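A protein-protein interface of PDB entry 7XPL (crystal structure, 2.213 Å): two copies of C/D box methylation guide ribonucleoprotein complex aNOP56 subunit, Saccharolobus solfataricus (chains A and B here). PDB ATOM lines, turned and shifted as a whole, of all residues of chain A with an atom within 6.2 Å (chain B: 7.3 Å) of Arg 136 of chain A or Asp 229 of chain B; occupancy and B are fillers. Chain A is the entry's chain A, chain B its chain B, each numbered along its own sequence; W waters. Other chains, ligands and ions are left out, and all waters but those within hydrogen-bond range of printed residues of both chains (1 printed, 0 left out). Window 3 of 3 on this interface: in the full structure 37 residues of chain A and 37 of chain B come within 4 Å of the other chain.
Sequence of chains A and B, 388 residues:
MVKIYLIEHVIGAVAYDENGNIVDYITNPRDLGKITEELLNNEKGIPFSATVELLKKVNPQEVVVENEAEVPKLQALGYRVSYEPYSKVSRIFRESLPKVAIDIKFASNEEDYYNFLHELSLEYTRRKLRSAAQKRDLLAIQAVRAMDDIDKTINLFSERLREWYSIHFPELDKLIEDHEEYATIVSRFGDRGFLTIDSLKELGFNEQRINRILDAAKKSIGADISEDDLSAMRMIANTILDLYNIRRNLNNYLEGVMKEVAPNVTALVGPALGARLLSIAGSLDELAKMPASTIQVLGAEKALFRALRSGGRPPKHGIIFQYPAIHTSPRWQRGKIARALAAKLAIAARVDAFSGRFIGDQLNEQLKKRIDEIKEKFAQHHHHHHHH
Printed residues of chain B within 4 Å of Gln 134 of chain A: Asp 224. Of chain B, only Asp 229 comes within 4 Å of Arg 136 of chain A. Trp 164 of chain B touches none of the printed residues of chain A. Glu 227 of chain B touches none of the printed residues of chain A. Of the printed residues of chain A, Asp 228 of chain B touches Tyr 253 (3.6 Å). Of the printed residues of chain A, Ala 232 of chain B touches Tyr 253. The nearest residue of chain B that does not touch Arg 136 of chain A is Ser 226 of chain B (5.2 Å). The nearest residue of chain A that does not touch Asp 229 of chain B is Val 257 of chain A (4.5 Å). The nearest printed residue of chain A that does not touch Ala 232 of chain B is Leu 139 of chain A (7.3 Å).
Water W1 lies within hydrogen-bond range of the side-chain hydroxyl of Tyr 253 of chain A (2.8 Å), the indole nitrogen of Trp 164 of chain B (2.8 Å) and the backbone carbonyl oxygen of Asp 229 of chain B (3.2 Å).
No position is printed for both chains.
The side-chain carboxylate (OD2) of Asp 229 of chain B sits at hydrogen-bond distance from the side-chain hydroxyl (OG) of Ser 226 of chain B (3.0 Å). The guanidinium group (NE) of Arg 136 of chain A lies within salt-bridge range of the side-chain carboxylate (OE1) of Glu 260 of chain A, at 2.7 Å. OG of Ser 226 of chain B is in hydrogen-bond range of N of Asp 228 of chain B, 3.3 Å away.
Printed residues of chain B that touch a printed residue of chain A: Ile 167, Asp 224, Asp 228, Asp 229 and Ala 232. Hydrophobic or aromatic side chains of chain A within 4 Å of the printed part of chain B: Ala 133, Leu 138, Leu 139 and Tyr 253.
NE2 of Gln 134 of chain A lies within hydrogen-bond range of O of Asp 224 of chain B (3.1 Å). OH of Tyr 253 of chain A lies within hydrogen-bond range of OD1 of Asp 229 of chain B, at 2.4 Å. NH1 of Arg 136 of chain A is in salt-bridge range of OD2 of Asp 229 of chain B, at 2.9 Å.
Ile 167 of chain B touches Ala 133 of chain A. CD1 of Ile 167 of chain B touches CB of Leu 138 of chain A, at 3.8 Å. Leu 139 of chain A touches Ile 167 of chain B (CD2 to CD1, 3.7 Å). Leu 139 of chain A touches Asp 229 of chain B (CD1 to OD2, 3.5 Å). O of Asp 228 of chain B touches CE1 of Tyr 253 of chain A, 3.6 Å away. Ala 232 of chain B touches Tyr 253 of chain A.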
ATOM      1  N   ALA A 133      21.394  18.073  16.344  1.00  0.00           N
ATOM      2  CA  ALA A 133      22.250  17.654  15.245  1.00  0.00           C
ATOM      3  C   ALA A 133      21.440  17.309  14.011  1.00  0.00           C
ATOM      4  O   ALA A 133      21.969  17.346  12.896  1.00  0.00           O
ATOM      5  CB  ALA A 133      23.095  16.449  15.679  1.00  0.00           C
ATOM      6  N   GLN A 134      20.159  17.004  14.193  1.00  0.00           N
ATOM      7  CA  GLN A 134      19.252  16.664  13.109  1.00  0.00           C
ATOM      8  C   GLN A 134      18.794  17.875  12.283  1.00  0.00           C
ATOM      9  O   GLN A 134      18.238  17.680  11.200  1.00  0.00           O
ATOM     10  CB  GLN A 134      18.047  15.919  13.710  1.00  0.00           C
ATOM     11  CG  GLN A 134      17.221  15.129  12.713  1.00  0.00           C
ATOM     12  CD  GLN A 134      18.067  14.106  11.933  1.00  0.00           C
ATOM     13  OE1 GLN A 134      18.671  13.188  12.528  1.00  0.00           O
ATOM     14  NE2 GLN A 134      18.107  14.257  10.596  1.00  0.00           N
ATOM     15  N   LYS A 135      19.046  19.109  12.734  1.00  0.00           N
ATOM     16  CA  LYS A 135      18.621  20.289  11.976  1.00  0.00           C
ATOM     17  C   LYS A 135      19.319  20.368  10.621  1.00  0.00           C
ATOM     18  O   LYS A 135      20.548  20.366  10.527  1.00  0.00           O
ATOM     19  CB  LYS A 135      18.901  21.570  12.755  1.00  0.00           C
ATOM     20  CG  LYS A 135      18.116  21.721  14.076  1.00  0.00           C
ATOM     21  CD  LYS A 135      16.679  22.180  13.859  1.00  0.00           C
ATOM     22  CE  LYS A 135      16.622  23.553  13.184  1.00  0.00           C
ATOM     23  NZ  LYS A 135      15.222  24.067  12.869  1.00  0.00           N
ATOM     24  N   ARG A 136      18.520  20.509   9.569  1.00  0.00           N
ATOM     25  CA  ARG A 136      19.053  20.504   8.218  1.00  0.00           C
ATOM     26  C   ARG A 136      19.942  21.717   7.927  1.00  0.00           C
ATOM     27  O   ARG A 136      20.848  21.625   7.091  1.00  0.00           O
ATOM     28  CB  ARG A 136      17.893  20.427   7.227  1.00  0.00           C
ATOM     29  CG  ARG A 136      17.120  19.118   7.311  1.00  0.00           C
ATOM     30  CD  ARG A 136      17.916  17.966   6.716  1.00  0.00           C
ATOM     31  NE  ARG A 136      18.008  18.070   5.262  1.00  0.00           N
ATOM     32  CZ  ARG A 136      18.932  17.457   4.526  1.00  0.00           C
ATOM     33  NH1 ARG A 136      19.843  16.695   5.121  1.00  0.00           N
ATOM     34  NH2 ARG A 136      18.952  17.618   3.198  1.00  0.00           N
ATOM     35  N   ASP A 137      19.717  22.853   8.590  1.00  0.00           N
ATOM     36  CA  ASP A 137      20.559  24.008   8.306  1.00  0.00           C
ATOM     37  C   ASP A 137      22.014  23.803   8.732  1.00  0.00           C
ATOM     38  O   ASP A 137      22.890  24.472   8.180  1.00  0.00           O
ATOM     39  CB  ASP A 137      19.991  25.292   8.956  1.00  0.00           C
ATOM     40  CG  ASP A 137      19.940  25.244  10.505  1.00  0.00           C
ATOM     41  OD1 ASP A 137      20.136  24.167  11.110  1.00  0.00           O
ATOM     42  OD2 ASP A 137      19.673  26.314  11.114  1.00  0.00           O
ATOM     43  N   LEU A 138      22.293  22.931   9.715  1.00  0.00           N
ATOM     44  CA  LEU A 138      23.696  22.619  10.034  1.00  0.00           C
ATOM     45  C   LEU A 138      24.481  22.171   8.800  1.00  0.00           C
ATOM     46  O   LEU A 138      25.655  22.525   8.636  1.00  0.00           O
ATOM     47  CB  LEU A 138      23.784  21.531  11.110  1.00  0.00           C
ATOM     48  CG  LEU A 138      23.253  21.874  12.497  1.00  0.00           C
ATOM     49  CD1 LEU A 138      23.648  20.793  13.478  1.00  0.00           C
ATOM     50  CD2 LEU A 138      23.733  23.260  12.938  1.00  0.00           C
ATOM     51  N   LEU A 139      23.850  21.389   7.924  1.00  0.00           N
ATOM     52  CA  LEU A 139      24.559  20.864   6.764  1.00  0.00           C
ATOM     53  C   LEU A 139      24.927  21.970   5.786  1.00  0.00           C
ATOM     54  O   LEU A 139      26.052  21.999   5.272  1.00  0.00           O
ATOM     55  CB  LEU A 139      23.712  19.790   6.089  1.00  0.00           C
ATOM     56  CG  LEU A 139      23.508  18.616   7.047  1.00  0.00           C
ATOM     57  CD1 LEU A 139      22.776  17.484   6.343  1.00  0.00           C
ATOM     58  CD2 LEU A 139      24.863  18.157   7.563  1.00  0.00           C
ATOM     59  N   ALA A 140      23.995  22.884   5.507  1.00  0.00           N
ATOM     60  CA  ALA A 140      24.312  24.014   4.639  1.00  0.00           C
ATOM     61  C   ALA A 140      25.450  24.844   5.208  1.00  0.00           C
ATOM     62  O   ALA A 140      26.290  25.360   4.461  1.00  0.00           O
ATOM     63  CB  ALA A 140      23.078  24.910   4.438  1.00  0.00           C
ATOM     64  N   ILE A 141      25.455  25.038   6.525  1.00  0.00           N
ATOM     65  CA  ILE A 141      26.469  25.883   7.131  1.00  0.00           C
ATOM     66  C   ILE A 141      27.855  25.251   6.998  1.00  0.00           C
ATOM     67  O   ILE A 141      28.815  25.933   6.625  1.00  0.00           O
ATOM     68  CB  ILE A 141      26.100  26.167   8.595  1.00  0.00           C
ATOM     69  CG1 ILE A 141      24.930  27.155   8.642  1.00  0.00           C
ATOM     70  CG2 ILE A 141      27.315  26.666   9.362  1.00  0.00           C
ATOM     71  CD1 ILE A 141      24.456  27.418  10.044  1.00  0.00           C
ATOM     72  N   TYR A 253      25.839  20.669  -4.427  1.00  0.00           N
ATOM     73  CA  TYR A 253      25.238  20.163  -3.198  1.00  0.00           C
ATOM     74  C   TYR A 253      24.541  21.285  -2.432  1.00  0.00           C
ATOM     75  O   TYR A 253      23.384  21.144  -2.009  1.00  0.00           O
ATOM     76  CB  TYR A 253      26.294  19.498  -2.331  1.00  0.00           C
ATOM     77  CG  TYR A 253      25.794  19.084  -0.962  1.00  0.00           C
ATOM     78  CD1 TYR A 253      25.080  17.903  -0.790  1.00  0.00           C
ATOM     79  CD2 TYR A 253      26.057  19.868   0.166  1.00  0.00           C
ATOM     80  CE1 TYR A 253      24.613  17.522   0.465  1.00  0.00           C
ATOM     81  CE2 TYR A 253      25.599  19.488   1.428  1.00  0.00           C
ATOM     82  CZ  TYR A 253      24.871  18.317   1.561  1.00  0.00           C
ATOM     83  OH  TYR A 253      24.423  17.928   2.790  1.00  0.00           O
ATOM     84  N   GLY A 256      21.027  22.193  -3.530  1.00  0.00           N
ATOM     85  CA  GLY A 256      19.977  21.301  -3.063  1.00  0.00           C
ATOM     86  C   GLY A 256      19.560  21.574  -1.630  1.00  0.00           C
ATOM     87  O   GLY A 256      18.368  21.649  -1.320  1.00  0.00           O
ATOM     88  N   VAL A 257      20.534  21.742  -0.736  1.00  0.00           N
ATOM     89  CA  VAL A 257      20.194  21.913   0.675  1.00  0.00           C
ATOM     90  C   VAL A 257      19.495  23.249   0.911  1.00  0.00           C
ATOM     91  O   VAL A 257      18.526  23.332   1.683  1.00  0.00           O
ATOM     92  CB  VAL A 257      21.454  21.768   1.546  1.00  0.00           C
ATOM     93  CG1 VAL A 257      21.178  22.203   2.972  1.00  0.00           C
ATOM     94  CG2 VAL A 257      21.926  20.334   1.523  1.00  0.00           C
ATOM     95  N   GLU A 260      15.894  23.657  -0.011  1.00  0.00           N
ATOM     96  CA  GLU A 260      15.028  22.998   0.958  1.00  0.00           C
ATOM     97  C   GLU A 260      15.014  23.711   2.307  1.00  0.00           C
ATOM     98  O   GLU A 260      13.959  23.817   2.950  1.00  0.00           O
ATOM     99  CB  GLU A 260      15.460  21.547   1.139  1.00  0.00           C
ATOM    100  CG  GLU A 260      15.065  20.949   2.495  1.00  0.00           C
ATOM    101  CD  GLU A 260      16.046  19.882   2.957  1.00  0.00           C
ATOM    102  OE1 GLU A 260      15.927  19.422   4.125  1.00  0.00           O
ATOM    103  OE2 GLU A 260      16.937  19.516   2.142  1.00  0.00           O
ATOM    104  N   VAL A 261      16.158  24.241   2.730  1.00  0.00           N
ATOM    105  CA  VAL A 261      16.269  24.804   4.069  1.00  0.00           C
ATOM    106  C   VAL A 261      15.813  26.263   4.108  1.00  0.00           C
ATOM    107  O   VAL A 261      15.166  26.686   5.068  1.00  0.00           O
ATOM    108  CB  VAL A 261      17.714  24.627   4.577  1.00  0.00           C
ATOM    109  CG1 VAL A 261      17.977  25.505   5.789  1.00  0.00           C
ATOM    110  CG2 VAL A 261      17.940  23.177   4.937  1.00  0.00           C
ATOM    111  N   TRP B 164      32.157  18.940  10.561  1.00  0.00           N
ATOM    112  CA  TRP B 164      31.099  18.569   9.637  1.00  0.00           C
ATOM    113  C   TRP B 164      30.660  17.126   9.857  1.00  0.00           C
ATOM    114  O   TRP B 164      29.460  16.828   9.909  1.00  0.00           O
ATOM    115  CB  TRP B 164      31.592  18.811   8.214  1.00  0.00           C
ATOM    116  CG  TRP B 164      30.553  18.720   7.143  1.00  0.00           C
ATOM    117  CD1 TRP B 164      29.232  18.410   7.292  1.00  0.00           C
ATOM    118  CD2 TRP B 164      30.757  18.954   5.751  1.00  0.00           C
ATOM    119  NE1 TRP B 164      28.608  18.425   6.077  1.00  0.00           N
ATOM    120  CE2 TRP B 164      29.522  18.759   5.111  1.00  0.00           C
ATOM    121  CE3 TRP B 164      31.875  19.303   4.978  1.00  0.00           C
ATOM    122  CZ2 TRP B 164      29.365  18.910   3.733  1.00  0.00           C
ATOM    123  CZ3 TRP B 164      31.722  19.448   3.612  1.00  0.00           C
ATOM    124  CH2 TRP B 164      30.472  19.255   3.002  1.00  0.00           C
ATOM    125  N   ILE B 167      28.548  16.000  13.101  1.00  0.00           N
ATOM    126  CA  ILE B 167      27.083  16.058  13.079  1.00  0.00           C
ATOM    127  C   ILE B 167      26.507  14.653  13.052  1.00  0.00           C
ATOM    128  O   ILE B 167      25.446  14.386  13.640  1.00  0.00           O
ATOM    129  CB  ILE B 167      26.585  16.874  11.863  1.00  0.00           C
ATOM    130  CG1 ILE B 167      26.895  18.359  12.005  1.00  0.00           C
ATOM    131  CG2 ILE B 167      25.066  16.685  11.608  1.00  0.00           C
ATOM    132  CD1 ILE B 167      26.614  19.092  10.708  1.00  0.00           C
ATOM    133  N   ASP B 224      21.032  10.975  11.897  1.00  0.00           N
ATOM    134  CA  ASP B 224      20.933  10.200  10.667  1.00  0.00           C
ATOM    135  C   ASP B 224      20.889  11.172   9.501  1.00  0.00           C
ATOM    136  O   ASP B 224      20.009  12.032   9.443  1.00  0.00           O
ATOM    137  CB  ASP B 224      19.686   9.317  10.653  1.00  0.00           C
ATOM    138  CG  ASP B 224      19.691   8.292  11.755  1.00  0.00           C
ATOM    139  OD1 ASP B 224      20.720   8.186  12.467  1.00  0.00           O
ATOM    140  OD2 ASP B 224      18.671   7.584  11.899  1.00  0.00           O
ATOM    141  N   ILE B 225      21.830  11.046   8.575  1.00  0.00           N
ATOM    142  CA  ILE B 225      21.859  11.920   7.413  1.00  0.00           C
ATOM    143  C   ILE B 225      21.774  11.055   6.160  1.00  0.00           C
ATOM    144  O   ILE B 225      21.864   9.829   6.215  1.00  0.00           O
ATOM    145  CB  ILE B 225      23.109  12.823   7.394  1.00  0.00           C
ATOM    146  CG1 ILE B 225      24.357  12.004   7.131  1.00  0.00           C
ATOM    147  CG2 ILE B 225      23.279  13.560   8.737  1.00  0.00           C
ATOM    148  CD1 ILE B 225      25.548  12.877   6.909  1.00  0.00           C
ATOM    149  N   SER B 226      21.597  11.713   5.021  1.00  0.00           N
ATOM    150  CA  SER B 226      21.449  10.977   3.779  1.00  0.00           C
ATOM    151  C   SER B 226      22.812  10.575   3.204  1.00  0.00           C
ATOM    152  O   SER B 226      23.883  10.936   3.710  1.00  0.00           O
ATOM    153  CB  SER B 226      20.686  11.804   2.758  1.00  0.00           C
ATOM    154  OG  SER B 226      21.553  12.760   2.194  1.00  0.00           O
ATOM    155  N   GLU B 227      22.752   9.802   2.124  1.00  0.00           N
ATOM    156  CA  GLU B 227      23.975   9.386   1.451  1.00  0.00           C
ATOM    157  C   GLU B 227      24.614  10.557   0.726  1.00  0.00           C
ATOM    158  O   GLU B 227      25.845  10.686   0.700  1.00  0.00           O
ATOM    159  CB  GLU B 227      23.670   8.253   0.481  1.00  0.00           C
ATOM    160  CG  GLU B 227      24.859   7.820  -0.388  1.00  0.00           C
ATOM    161  CD  GLU B 227      24.600   6.505  -1.117  1.00  0.00           C
ATOM    162  OE1 GLU B 227      23.424   6.061  -1.123  1.00  0.00           O
ATOM    163  OE2 GLU B 227      25.568   5.919  -1.673  1.00  0.00           O
ATOM    164  N   ASP B 228      23.797  11.431   0.142  1.00  0.00           N
ATOM    165  CA  ASP B 228      24.331  12.630  -0.495  1.00  0.00           C
ATOM    166  C   ASP B 228      25.006  13.547   0.519  1.00  0.00           C
ATOM    167  O   ASP B 228      26.009  14.197   0.201  1.00  0.00           O
ATOM    168  CB  ASP B 228      23.217  13.381  -1.221  1.00  0.00           C
ATOM    169  CG  ASP B 228      22.417  12.482  -2.138  1.00  0.00           C
ATOM    170  OD1 ASP B 228      23.006  12.035  -3.156  1.00  0.00           O
ATOM    171  OD2 ASP B 228      21.212  12.241  -1.843  1.00  0.00           O
ATOM    172  N   ASP B 229      24.444  13.652   1.731  1.00  0.00           N
ATOM    173  CA  ASP B 229      25.097  14.451   2.764  1.00  0.00           C
ATOM    174  C   ASP B 229      26.444  13.848   3.117  1.00  0.00           C
ATOM    175  O   ASP B 229      27.459  14.552   3.180  1.00  0.00           O
ATOM    176  CB  ASP B 229      24.221  14.556   4.009  1.00  0.00           C
ATOM    177  CG  ASP B 229      22.881  15.205   3.730  1.00  0.00           C
ATOM    178  OD1 ASP B 229      22.819  16.127   2.880  1.00  0.00           O
ATOM    179  OD2 ASP B 229      21.890  14.784   4.367  1.00  0.00           O
ATOM    180  N   LEU B 230      26.474  12.528   3.320  1.00  0.00           N
ATOM    181  CA  LEU B 230      27.734  11.859   3.597  1.00  0.00           C
ATOM    182  C   LEU B 230      28.723  12.068   2.461  1.00  0.00           C
ATOM    183  O   LEU B 230      29.913  12.274   2.711  1.00  0.00           O
ATOM    184  CB  LEU B 230      27.498  10.374   3.862  1.00  0.00           C
ATOM    185  CG  LEU B 230      26.894  10.103   5.246  1.00  0.00           C
ATOM    186  CD1 LEU B 230      26.214   8.728   5.326  1.00  0.00           C
ATOM    187  CD2 LEU B 230      27.924  10.264   6.380  1.00  0.00           C
ATOM    188  N   SER B 231      28.244  12.079   1.210  1.00  0.00           N
ATOM    189  CA  SER B 231      29.178  12.174   0.089  1.00  0.00           C
ATOM    190  C   SER B 231      29.810  13.553  -0.018  1.00  0.00           C
ATOM    191  O   SER B 231      30.949  13.672  -0.473  1.00  0.00           O
ATOM    192  CB  SER B 231      28.490  11.819  -1.225  1.00  0.00           C
ATOM    193  OG  SER B 231      27.982  10.505  -1.135  1.00  0.00           O
ATOM    194  N   ALA B 232      29.099  14.605   0.386  1.00  0.00           N
ATOM    195  CA  ALA B 232      29.735  15.917   0.408  1.00  0.00           C
ATOM    196  C   ALA B 232      30.881  15.937   1.415  1.00  0.00           C
ATOM    197  O   ALA B 232      31.915  16.567   1.174  1.00  0.00           O
ATOM    198  CB  ALA B 232      28.701  17.009   0.717  1.00  0.00           C
ATOM    199  N   MET B 233      30.723  15.232   2.539  1.00  0.00           N
ATOM    200  CA  MET B 233      31.788  15.161   3.538  1.00  0.00           C
ATOM    201  C   MET B 233      32.984  14.351   3.037  1.00  0.00           C
ATOM    202  O   MET B 233      34.141  14.728   3.272  1.00  0.00           O
ATOM    203  CB  MET B 233      31.259  14.546   4.829  1.00  0.00           C
ATOM    204  CG  MET B 233      29.973  15.176   5.373  1.00  0.00           C
ATOM    205  SD  MET B 233      29.423  14.248   6.818  1.00  0.00           S
ATOM    206  CE  MET B 233      28.028  15.269   7.360  1.00  0.00           C
ATOM    207  N   ARG B 234      32.723  13.225   2.364  1.00  0.00           N
ATOM    208  CA  ARG B 234      33.796  12.367   1.873  1.00  0.00           C
ATOM    209  C   ARG B 234      34.644  13.046   0.809  1.00  0.00           C
ATOM    210  O   ARG B 234      35.796  12.649   0.603  1.00  0.00           O
ATOM    211  CB  ARG B 234      33.201  11.068   1.330  1.00  0.00           C
ATOM    212  CG  ARG B 234      32.434  10.302   2.410  1.00  0.00           C
ATOM    213  CD  ARG B 234      31.579   9.173   1.841  1.00  0.00           C
ATOM    214  NE  ARG B 234      32.325   7.921   1.773  1.00  0.00           N
ATOM    215  CZ  ARG B 234      31.778   6.724   1.587  1.00  0.00           C
ATOM    216  NH1 ARG B 234      30.467   6.591   1.454  1.00  0.00           N
ATOM    217  NH2 ARG B 234      32.546   5.650   1.552  1.00  0.00           N
HETATM  218  O   HOH W   1      26.592  17.376   4.430  1.00  0.00           O
